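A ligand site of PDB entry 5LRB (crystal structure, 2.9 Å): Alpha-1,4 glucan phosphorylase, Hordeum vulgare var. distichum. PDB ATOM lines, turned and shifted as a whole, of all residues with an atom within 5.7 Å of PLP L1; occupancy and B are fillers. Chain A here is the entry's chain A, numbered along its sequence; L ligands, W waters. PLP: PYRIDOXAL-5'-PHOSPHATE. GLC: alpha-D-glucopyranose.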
ATOM      1  N   LEU A  95      -5.692  11.562   1.711  1.00  0.00           N
ATOM      2  CA  LEU A  95      -5.615  12.547   0.627  1.00  0.00           C
ATOM      3  C   LEU A  95      -5.067  11.861  -0.630  1.00  0.00           C
ATOM      4  O   LEU A  95      -3.945  12.116  -1.034  1.00  0.00           O
ATOM      5  CB  LEU A  95      -4.739  13.754   1.004  1.00  0.00           C
ATOM      6  CG  LEU A  95      -5.370  15.161   1.201  1.00  0.00           C
ATOM      7  CD1 LEU A  95      -4.342  16.239   0.890  1.00  0.00           C
ATOM      8  CD2 LEU A  95      -6.616  15.394   0.361  1.00  0.00           C
ATOM      9  N   ASN A 138      -7.734  15.767   3.923  1.00  0.00           N
ATOM     10  CA  ASN A 138      -7.625  17.193   4.102  1.00  0.00           C
ATOM     11  C   ASN A 138      -6.170  17.662   4.107  1.00  0.00           C
ATOM     12  O   ASN A 138      -5.730  18.329   3.158  1.00  0.00           O
ATOM     13  CB  ASN A 138      -8.310  17.596   5.412  1.00  0.00           C
ATOM     14  CG  ASN A 138      -8.137  19.066   5.729  1.00  0.00           C
ATOM     15  OD1 ASN A 138      -8.052  19.451   6.900  1.00  0.00           O
ATOM     16  ND2 ASN A 138      -8.106  19.902   4.692  1.00  0.00           N
ATOM     17  N   GLY A 139      -5.446  17.306   5.158  1.00  0.00           N
ATOM     18  CA  GLY A 139      -4.091  17.801   5.385  1.00  0.00           C
ATOM     19  C   GLY A 139      -3.054  16.696   5.458  1.00  0.00           C
ATOM     20  O   GLY A 139      -3.262  15.599   4.921  1.00  0.00           O
ATOM     21  N   GLY A 140      -1.938  17.000   6.121  1.00  0.00           N
ATOM     22  CA  GLY A 140      -0.777  16.123   6.185  1.00  0.00           C
ATOM     23  C   GLY A 140      -1.079  14.694   6.607  1.00  0.00           C
ATOM     24  O   GLY A 140      -0.563  13.753   6.014  1.00  0.00           O
ATOM     25  N   ARG A 143      -2.332  12.793   3.638  1.00  0.00           N
ATOM     26  CA  ARG A 143      -1.405  12.695   2.512  1.00  0.00           C
ATOM     27  C   ARG A 143      -0.251  11.787   2.888  1.00  0.00           C
ATOM     28  O   ARG A 143       0.230  11.036   2.052  1.00  0.00           O
ATOM     29  CB  ARG A 143      -0.905  14.074   2.120  1.00  0.00           C
ATOM     30  CG  ARG A 143      -0.026  14.143   0.886  1.00  0.00           C
ATOM     31  CD  ARG A 143      -0.639  13.501  -0.347  1.00  0.00           C
ATOM     32  NE  ARG A 143       0.074  12.282  -0.735  1.00  0.00           N
ATOM     33  CZ  ARG A 143      -0.261  11.478  -1.747  1.00  0.00           C
ATOM     34  NH1 ARG A 143      -1.325  11.734  -2.509  1.00  0.00           N
ATOM     35  NH2 ARG A 143       0.478  10.395  -1.991  1.00  0.00           N
ATOM     36  N   TRP A 578       5.758  12.975  -6.454  1.00  0.00           N
ATOM     37  CA  TRP A 578       6.215  14.310  -6.101  1.00  0.00           C
ATOM     38  C   TRP A 578       7.484  14.740  -6.811  1.00  0.00           C
ATOM     39  O   TRP A 578       7.942  15.855  -6.609  1.00  0.00           O
ATOM     40  CB  TRP A 578       6.325  14.452  -4.572  1.00  0.00           C
ATOM     41  CG  TRP A 578       4.959  14.308  -3.921  1.00  0.00           C
ATOM     42  CD1 TRP A 578       4.552  13.312  -3.080  1.00  0.00           C
ATOM     43  CD2 TRP A 578       3.820  15.158  -4.106  1.00  0.00           C
ATOM     44  NE1 TRP A 578       3.240  13.491  -2.721  1.00  0.00           N
ATOM     45  CE2 TRP A 578       2.763  14.621  -3.344  1.00  0.00           C
ATOM     46  CE3 TRP A 578       3.592  16.333  -4.830  1.00  0.00           C
ATOM     47  CZ2 TRP A 578       1.499  15.228  -3.286  1.00  0.00           C
ATOM     48  CZ3 TRP A 578       2.343  16.924  -4.779  1.00  0.00           C
ATOM     49  CH2 TRP A 578       1.319  16.370  -4.011  1.00  0.00           C
ATOM     50  N   VAL A 655       1.995  27.585   1.141  1.00  0.00           N
ATOM     51  CA  VAL A 655       0.818  26.828   0.800  1.00  0.00           C
ATOM     52  C   VAL A 655       0.591  25.810   1.933  1.00  0.00           C
ATOM     53  O   VAL A 655       1.321  24.826   2.049  1.00  0.00           O
ATOM     54  CB  VAL A 655       0.980  26.285  -0.652  1.00  0.00           C
ATOM     55  CG1 VAL A 655       1.250  24.790  -0.694  1.00  0.00           C
ATOM     56  CG2 VAL A 655      -0.210  26.658  -1.511  1.00  0.00           C
ATOM     57  N   LYS A 656      -0.363  26.116   2.808  1.00  0.00           N
ATOM     58  CA  LYS A 656      -0.751  25.256   3.943  1.00  0.00           C
ATOM     59  C   LYS A 656      -1.963  25.806   4.695  1.00  0.00           C
ATOM     60  O   LYS A 656      -2.335  26.956   4.507  1.00  0.00           O
ATOM     61  CB  LYS A 656       0.410  25.016   4.928  1.00  0.00           C
ATOM     62  CG  LYS A 656       1.242  26.238   5.320  1.00  0.00           C
ATOM     63  CD  LYS A 656       2.503  25.848   6.114  1.00  0.00           C
ATOM     64  CE  LYS A 656       3.685  25.432   5.233  1.00  0.00           C
ATOM     65  NZ  LYS A 656       3.742  23.986   4.843  1.00  0.00           N
ATOM     66  N   ARG A 657      -2.571  24.978   5.546  1.00  0.00           N
ATOM     67  CA  ARG A 657      -3.812  25.357   6.217  1.00  0.00           C
ATOM     68  C   ARG A 657      -3.661  26.728   6.898  1.00  0.00           C
ATOM     69  O   ARG A 657      -2.630  27.068   7.493  1.00  0.00           O
ATOM     70  CB  ARG A 657      -4.301  24.265   7.197  1.00  0.00           C
ATOM     71  CG  ARG A 657      -4.407  24.642   8.665  1.00  0.00           C
ATOM     72  CD  ARG A 657      -5.431  23.794   9.418  1.00  0.00           C
ATOM     73  NE  ARG A 657      -6.807  24.170   9.117  1.00  0.00           N
ATOM     74  CZ  ARG A 657      -7.579  23.533   8.236  1.00  0.00           C
ATOM     75  NH1 ARG A 657      -8.811  23.954   8.029  1.00  0.00           N
ATOM     76  NH2 ARG A 657      -7.126  22.497   7.570  1.00  0.00           N
ATOM     77  N   LYS A 662       0.523  28.932  11.998  1.00  0.00           N
ATOM     78  CA  LYS A 662       1.346  28.709  10.807  1.00  0.00           C
ATOM     79  C   LYS A 662       1.905  30.038  10.307  1.00  0.00           C
ATOM     80  O   LYS A 662       2.901  30.077   9.594  1.00  0.00           O
ATOM     81  CB  LYS A 662       0.531  28.019   9.709  1.00  0.00           C
ATOM     82  CG  LYS A 662      -0.093  26.695  10.161  1.00  0.00           C
ATOM     83  CD  LYS A 662       0.227  25.537   9.240  1.00  0.00           C
ATOM     84  CE  LYS A 662       0.143  24.235   9.999  1.00  0.00           C
ATOM     85  NZ  LYS A 662       0.087  23.014   9.148  1.00  0.00           N
ATOM     86  N   TYR A 740      -6.966  24.840  -2.610  1.00  0.00           N
ATOM     87  CA  TYR A 740      -5.699  24.124  -2.603  1.00  0.00           C
ATOM     88  C   TYR A 740      -5.929  22.647  -2.267  1.00  0.00           C
ATOM     89  O   TYR A 740      -6.608  22.312  -1.310  1.00  0.00           O
ATOM     90  CB  TYR A 740      -4.713  24.766  -1.623  1.00  0.00           C
ATOM     91  CG  TYR A 740      -3.434  23.990  -1.453  1.00  0.00           C
ATOM     92  CD1 TYR A 740      -2.476  23.953  -2.461  1.00  0.00           C
ATOM     93  CD2 TYR A 740      -3.174  23.297  -0.279  1.00  0.00           C
ATOM     94  CE1 TYR A 740      -1.292  23.240  -2.316  1.00  0.00           C
ATOM     95  CE2 TYR A 740      -1.997  22.577  -0.120  1.00  0.00           C
ATOM     96  CZ  TYR A 740      -1.052  22.538  -1.135  1.00  0.00           C
ATOM     97  OH  TYR A 740       0.121  21.824  -0.955  1.00  0.00           O
ATOM     98  N   ASN A 741      -5.373  21.781  -3.110  1.00  0.00           N
ATOM     99  CA  ASN A 741      -5.486  20.336  -2.928  1.00  0.00           C
ATOM    100  C   ASN A 741      -4.341  19.627  -3.667  1.00  0.00           C
ATOM    101  O   ASN A 741      -3.435  20.280  -4.207  1.00  0.00           O
ATOM    102  CB  ASN A 741      -6.860  19.846  -3.409  1.00  0.00           C
ATOM    103  CG  ASN A 741      -7.073  20.043  -4.899  1.00  0.00           C
ATOM    104  OD1 ASN A 741      -6.146  20.386  -5.638  1.00  0.00           O
ATOM    105  ND2 ASN A 741      -8.281  19.813  -5.342  1.00  0.00           N
ATOM    106  N   VAL A 742      -4.383  18.297  -3.688  1.00  0.00           N
ATOM    107  CA  VAL A 742      -3.284  17.518  -4.254  1.00  0.00           C
ATOM    108  C   VAL A 742      -2.969  17.972  -5.682  1.00  0.00           C
ATOM    109  O   VAL A 742      -1.814  18.169  -6.022  1.00  0.00           O
ATOM    110  CB  VAL A 742      -3.577  16.002  -4.227  1.00  0.00           C
ATOM    111  CG1 VAL A 742      -2.383  15.228  -4.761  1.00  0.00           C
ATOM    112  CG2 VAL A 742      -3.934  15.545  -2.825  1.00  0.00           C
ATOM    113  N   ALA A 745      -1.192  21.354  -5.685  1.00  0.00           N
ATOM    114  CA  ALA A 745       0.185  21.140  -5.246  1.00  0.00           C
ATOM    115  C   ALA A 745       1.053  20.556  -6.360  1.00  0.00           C
ATOM    116  O   ALA A 745       2.195  20.970  -6.541  1.00  0.00           O
ATOM    117  CB  ALA A 745       0.224  20.231  -4.039  1.00  0.00           C
ATOM    118  N   ILE A 749       4.136  22.986  -6.904  1.00  0.00           N
ATOM    119  CA  ILE A 749       5.375  22.626  -6.216  1.00  0.00           C
ATOM    120  C   ILE A 749       6.597  22.616  -7.121  1.00  0.00           C
ATOM    121  O   ILE A 749       7.595  23.240  -6.792  1.00  0.00           O
ATOM    122  CB  ILE A 749       5.231  21.283  -5.455  1.00  0.00           C
ATOM    123  CG1 ILE A 749       4.446  21.503  -4.166  1.00  0.00           C
ATOM    124  CG2 ILE A 749       6.599  20.666  -5.156  1.00  0.00           C
ATOM    125  CD1 ILE A 749       4.043  20.229  -3.447  1.00  0.00           C
ATOM    126  N   HIS A 757       7.968  27.906   5.440  1.00  0.00           N
ATOM    127  CA  HIS A 757       7.529  27.007   6.486  1.00  0.00           C
ATOM    128  C   HIS A 757       7.917  27.690   7.775  1.00  0.00           C
ATOM    129  O   HIS A 757       8.945  27.378   8.383  1.00  0.00           O
ATOM    130  CB  HIS A 757       8.208  25.638   6.321  1.00  0.00           C
ATOM    131  CG  HIS A 757       8.067  25.058   4.944  1.00  0.00           C
ATOM    132  ND1 HIS A 757       7.015  24.248   4.586  1.00  0.00           N
ATOM    133  CD2 HIS A 757       8.822  25.199   3.840  1.00  0.00           C
ATOM    134  CE1 HIS A 757       7.152  23.879   3.329  1.00  0.00           C
ATOM    135  NE2 HIS A 757       8.236  24.460   2.849  1.00  0.00           N
ATOM    136  N   GLU A 764       5.091  22.797  14.999  1.00  0.00           N
ATOM    137  CA  GLU A 764       4.910  21.826  13.928  1.00  0.00           C
ATOM    138  C   GLU A 764       5.629  20.532  14.327  1.00  0.00           C
ATOM    139  O   GLU A 764       6.761  20.602  14.832  1.00  0.00           O
ATOM    140  CB  GLU A 764       5.481  22.359  12.617  1.00  0.00           C
ATOM    141  CG  GLU A 764       4.755  21.895  11.363  1.00  0.00           C
ATOM    142  CD  GLU A 764       3.488  22.697  11.099  1.00  0.00           C
ATOM    143  OE1 GLU A 764       2.393  22.112  11.042  1.00  0.00           O
ATOM    144  OE2 GLU A 764       3.586  23.934  10.943  1.00  0.00           O
ATOM    145  N   GLY A 767       5.712  18.009   8.934  1.00  0.00           N
ATOM    146  CA  GLY A 767       5.512  18.723   7.673  1.00  0.00           C
ATOM    147  C   GLY A 767       5.985  17.878   6.493  1.00  0.00           C
ATOM    148  O   GLY A 767       7.154  17.517   6.418  1.00  0.00           O
ATOM    149  N   THR A 768       5.074  17.543   5.582  1.00  0.00           N
ATOM    150  CA  THR A 768       5.444  16.744   4.426  1.00  0.00           C
ATOM    151  C   THR A 768       5.688  17.599   3.197  1.00  0.00           C
ATOM    152  O   THR A 768       6.493  17.231   2.363  1.00  0.00           O
ATOM    153  CB  THR A 768       4.404  15.631   4.123  1.00  0.00           C
ATOM    154  OG1 THR A 768       3.088  16.167   4.029  1.00  0.00           O
ATOM    155  CG2 THR A 768       4.425  14.594   5.227  1.00  0.00           C
ATOM    156  N   SER A 769       5.007  18.746   3.083  1.00  0.00           N
ATOM    157  CA  SER A 769       5.205  19.623   1.919  1.00  0.00           C
ATOM    158  C   SER A 769       6.645  20.158   1.852  1.00  0.00           C
ATOM    159  O   SER A 769       7.196  20.345   0.761  1.00  0.00           O
ATOM    160  CB  SER A 769       4.181  20.772   1.880  1.00  0.00           C
ATOM    161  OG  SER A 769       4.412  21.734   2.907  1.00  0.00           O
ATOM    162  N   ASN A 770       7.249  20.387   3.023  1.00  0.00           N
ATOM    163  CA  ASN A 770       8.661  20.749   3.130  1.00  0.00           C
ATOM    164  C   ASN A 770       9.530  19.870   2.270  1.00  0.00           C
ATOM    165  O   ASN A 770      10.406  20.333   1.537  1.00  0.00           O
ATOM    166  CB  ASN A 770       9.154  20.556   4.568  1.00  0.00           C
ATOM    167  CG  ASN A 770       8.258  21.163   5.605  1.00  0.00           C
ATOM    168  OD1 ASN A 770       7.032  21.163   5.463  1.00  0.00           O
ATOM    169  ND2 ASN A 770       8.862  21.666   6.678  1.00  0.00           N
ATOM    170  N   LYS A 772       8.572  17.727  -0.130  1.00  0.00           N
ATOM    171  CA  LYS A 772       8.161  17.800  -1.540  1.00  0.00           C
ATOM    172  C   LYS A 772       8.878  18.921  -2.260  1.00  0.00           C
ATOM    173  O   LYS A 772       9.410  18.722  -3.342  1.00  0.00           O
ATOM    174  CB  LYS A 772       6.650  18.036  -1.664  1.00  0.00           C
ATOM    175  CG  LYS A 772       5.759  16.952  -1.073  1.00  0.00           C
ATOM    176  CD  LYS A 772       4.295  17.356  -1.117  1.00  0.00           C
ATOM    177  CE  LYS A 772       3.441  16.417  -0.283  1.00  0.00           C
ATOM    178  NZ  LYS A 772       2.084  16.986   0.006  1.00  0.00           N
HETATM  179  N1  PLP L   1      -2.051  19.502   1.474  1.00  0.00           N
HETATM  180  C2  PLP L   1      -1.728  18.928   0.293  1.00  0.00           C
HETATM  181  C2A PLP L   1      -2.667  19.025  -0.874  1.00  0.00           C
HETATM  182  C3  PLP L   1      -0.462  18.203   0.137  1.00  0.00           C
HETATM  183  O3  PLP L   1      -0.116  17.622  -1.023  1.00  0.00           O
HETATM  184  C4  PLP L   1       0.428  18.137   1.290  1.00  0.00           C
HETATM  185  C4A PLP L   1       1.700  17.407   1.142  1.00  0.00           C
HETATM  186  C5  PLP L   1      -0.023  18.812   2.537  1.00  0.00           C
HETATM  187  C6  PLP L   1      -1.247  19.460   2.551  1.00  0.00           C
HETATM  188  C5A PLP L   1       0.794  18.811   3.805  1.00  0.00           C
HETATM  189  O4P PLP L   1       1.596  19.976   3.895  1.00  0.00           O
HETATM  190  P   PLP L   1       2.094  20.436   5.362  1.00  0.00           P
HETATM  191  O1P PLP L   1       2.207  19.153   6.184  1.00  0.00           O
HETATM  192  O2P PLP L   1       3.417  21.117   5.112  1.00  0.00           O
HETATM  193  O3P PLP L   1       0.992  21.407   5.789  1.00  0.00           O
HETATM  194  C1  GLC L   2       3.059  15.881   9.358  1.00  0.00           C
HETATM  195  C2  GLC L   2       2.181  15.038  10.247  1.00  0.00           C
HETATM  196  C3  GLC L   2       0.804  15.712  10.322  1.00  0.00           C
HETATM  197  C4  GLC L   2       0.886  17.189  10.685  1.00  0.00           C
HETATM  198  C5  GLC L   2       2.001  17.907   9.918  1.00  0.00           C
HETATM  199  C6  GLC L   2       2.262  19.290  10.496  1.00  0.00           C
HETATM  200  O1  GLC L   2       2.475  15.948   8.074  1.00  0.00           O
HETATM  201  O2  GLC L   2       2.134  13.753   9.674  1.00  0.00           O
HETATM  202  O3  GLC L   2      -0.002  15.125  11.303  1.00  0.00           O
HETATM  203  O4  GLC L   2      -0.365  17.793  10.418  1.00  0.00           O
HETATM  204  O5  GLC L   2       3.193  17.153   9.971  1.00  0.00           O
HETATM  205  O6  GLC L   2       1.265  20.179  10.016  1.00  0.00           O
HETATM  206  O   HOH W   1      -0.991  20.079   7.526  1.00  0.00           O
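Leu 95 touches PLP L1.
Gly 140 touches PLP L1 (CA to C5A, 3.9 Å).
Arg 143 touches PLP L1.
Trp 578 touches PLP L1 (CH2 to O3, 3.5 Å).
Tyr 740 touches PLP L1.
Asn 741 touches PLP L1.
N of Val 742 touches C2A of PLP L1 (3.4 Å).
CA of Gly 767 touches O1P of PLP L1, at 3.7 Å.
Asn 770 touches PLP L1.
Hydrophobic or aromatic side chains that line PLP L1: Leu 95, Trp 578 and Tyr 740.
An oxygen (O3P) of PLP L1 lies within salt-bridge range of the side-chain amino group (NZ) of Lys 662.
The backbone NH (N) of Gly 767 lies within hydrogen-bond range of an oxygen (O5) of GLC L2 (2.9 Å).
OG of Ser 769 lies within hydrogen-bond range of O2P of PLP L1 (2.5 Å).
The side-chain carboxylate (OE1) of Glu 764 sits at hydrogen-bond distance from an oxygen (O6) of GLC L2.
The side-chain amino group (NZ) of Lys 656 is in salt-bridge range of an oxygen (O2P) of PLP L1 (2.9 Å).
The side-chain amino group of Lys 662 is in hydrogen-bond range of an oxygen (O6) of GLC L2, at 3.2 Å.
An oxygen (O1P) of PLP L1 is in hydrogen-bond range of the backbone NH of Thr 768 (3.3 Å).
The side-chain amino group (NZ) of Lys 772 is covalently linked to a carbon (C4A) of PLP L1, 1.3 Å away.
NZ of Lys 656 sits at hydrogen-bond distance from ND1 of His 757.
The backbone carbonyl oxygen (O) of Leu 95 sits at hydrogen-bond distance from the guanidinium group (NH1) of Arg 143, at 3.0 Å.
OE1 of Glu 764 lies within salt-bridge range of NZ of Lys 662 (3.1 Å).
ND1 of His 757 sits at hydrogen-bond distance from OD1 of Asn 770 (3.2 Å).
The side-chain hydroxyl (OG) of Ser 769 lies within hydrogen-bond range of the side-chain amino group (NZ) of Lys 656.
Water W1 bridges an oxygen (O3P) of PLP L1 (3.0 Å) and an oxygen (O6) of GLC L2 (3.4 Å).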
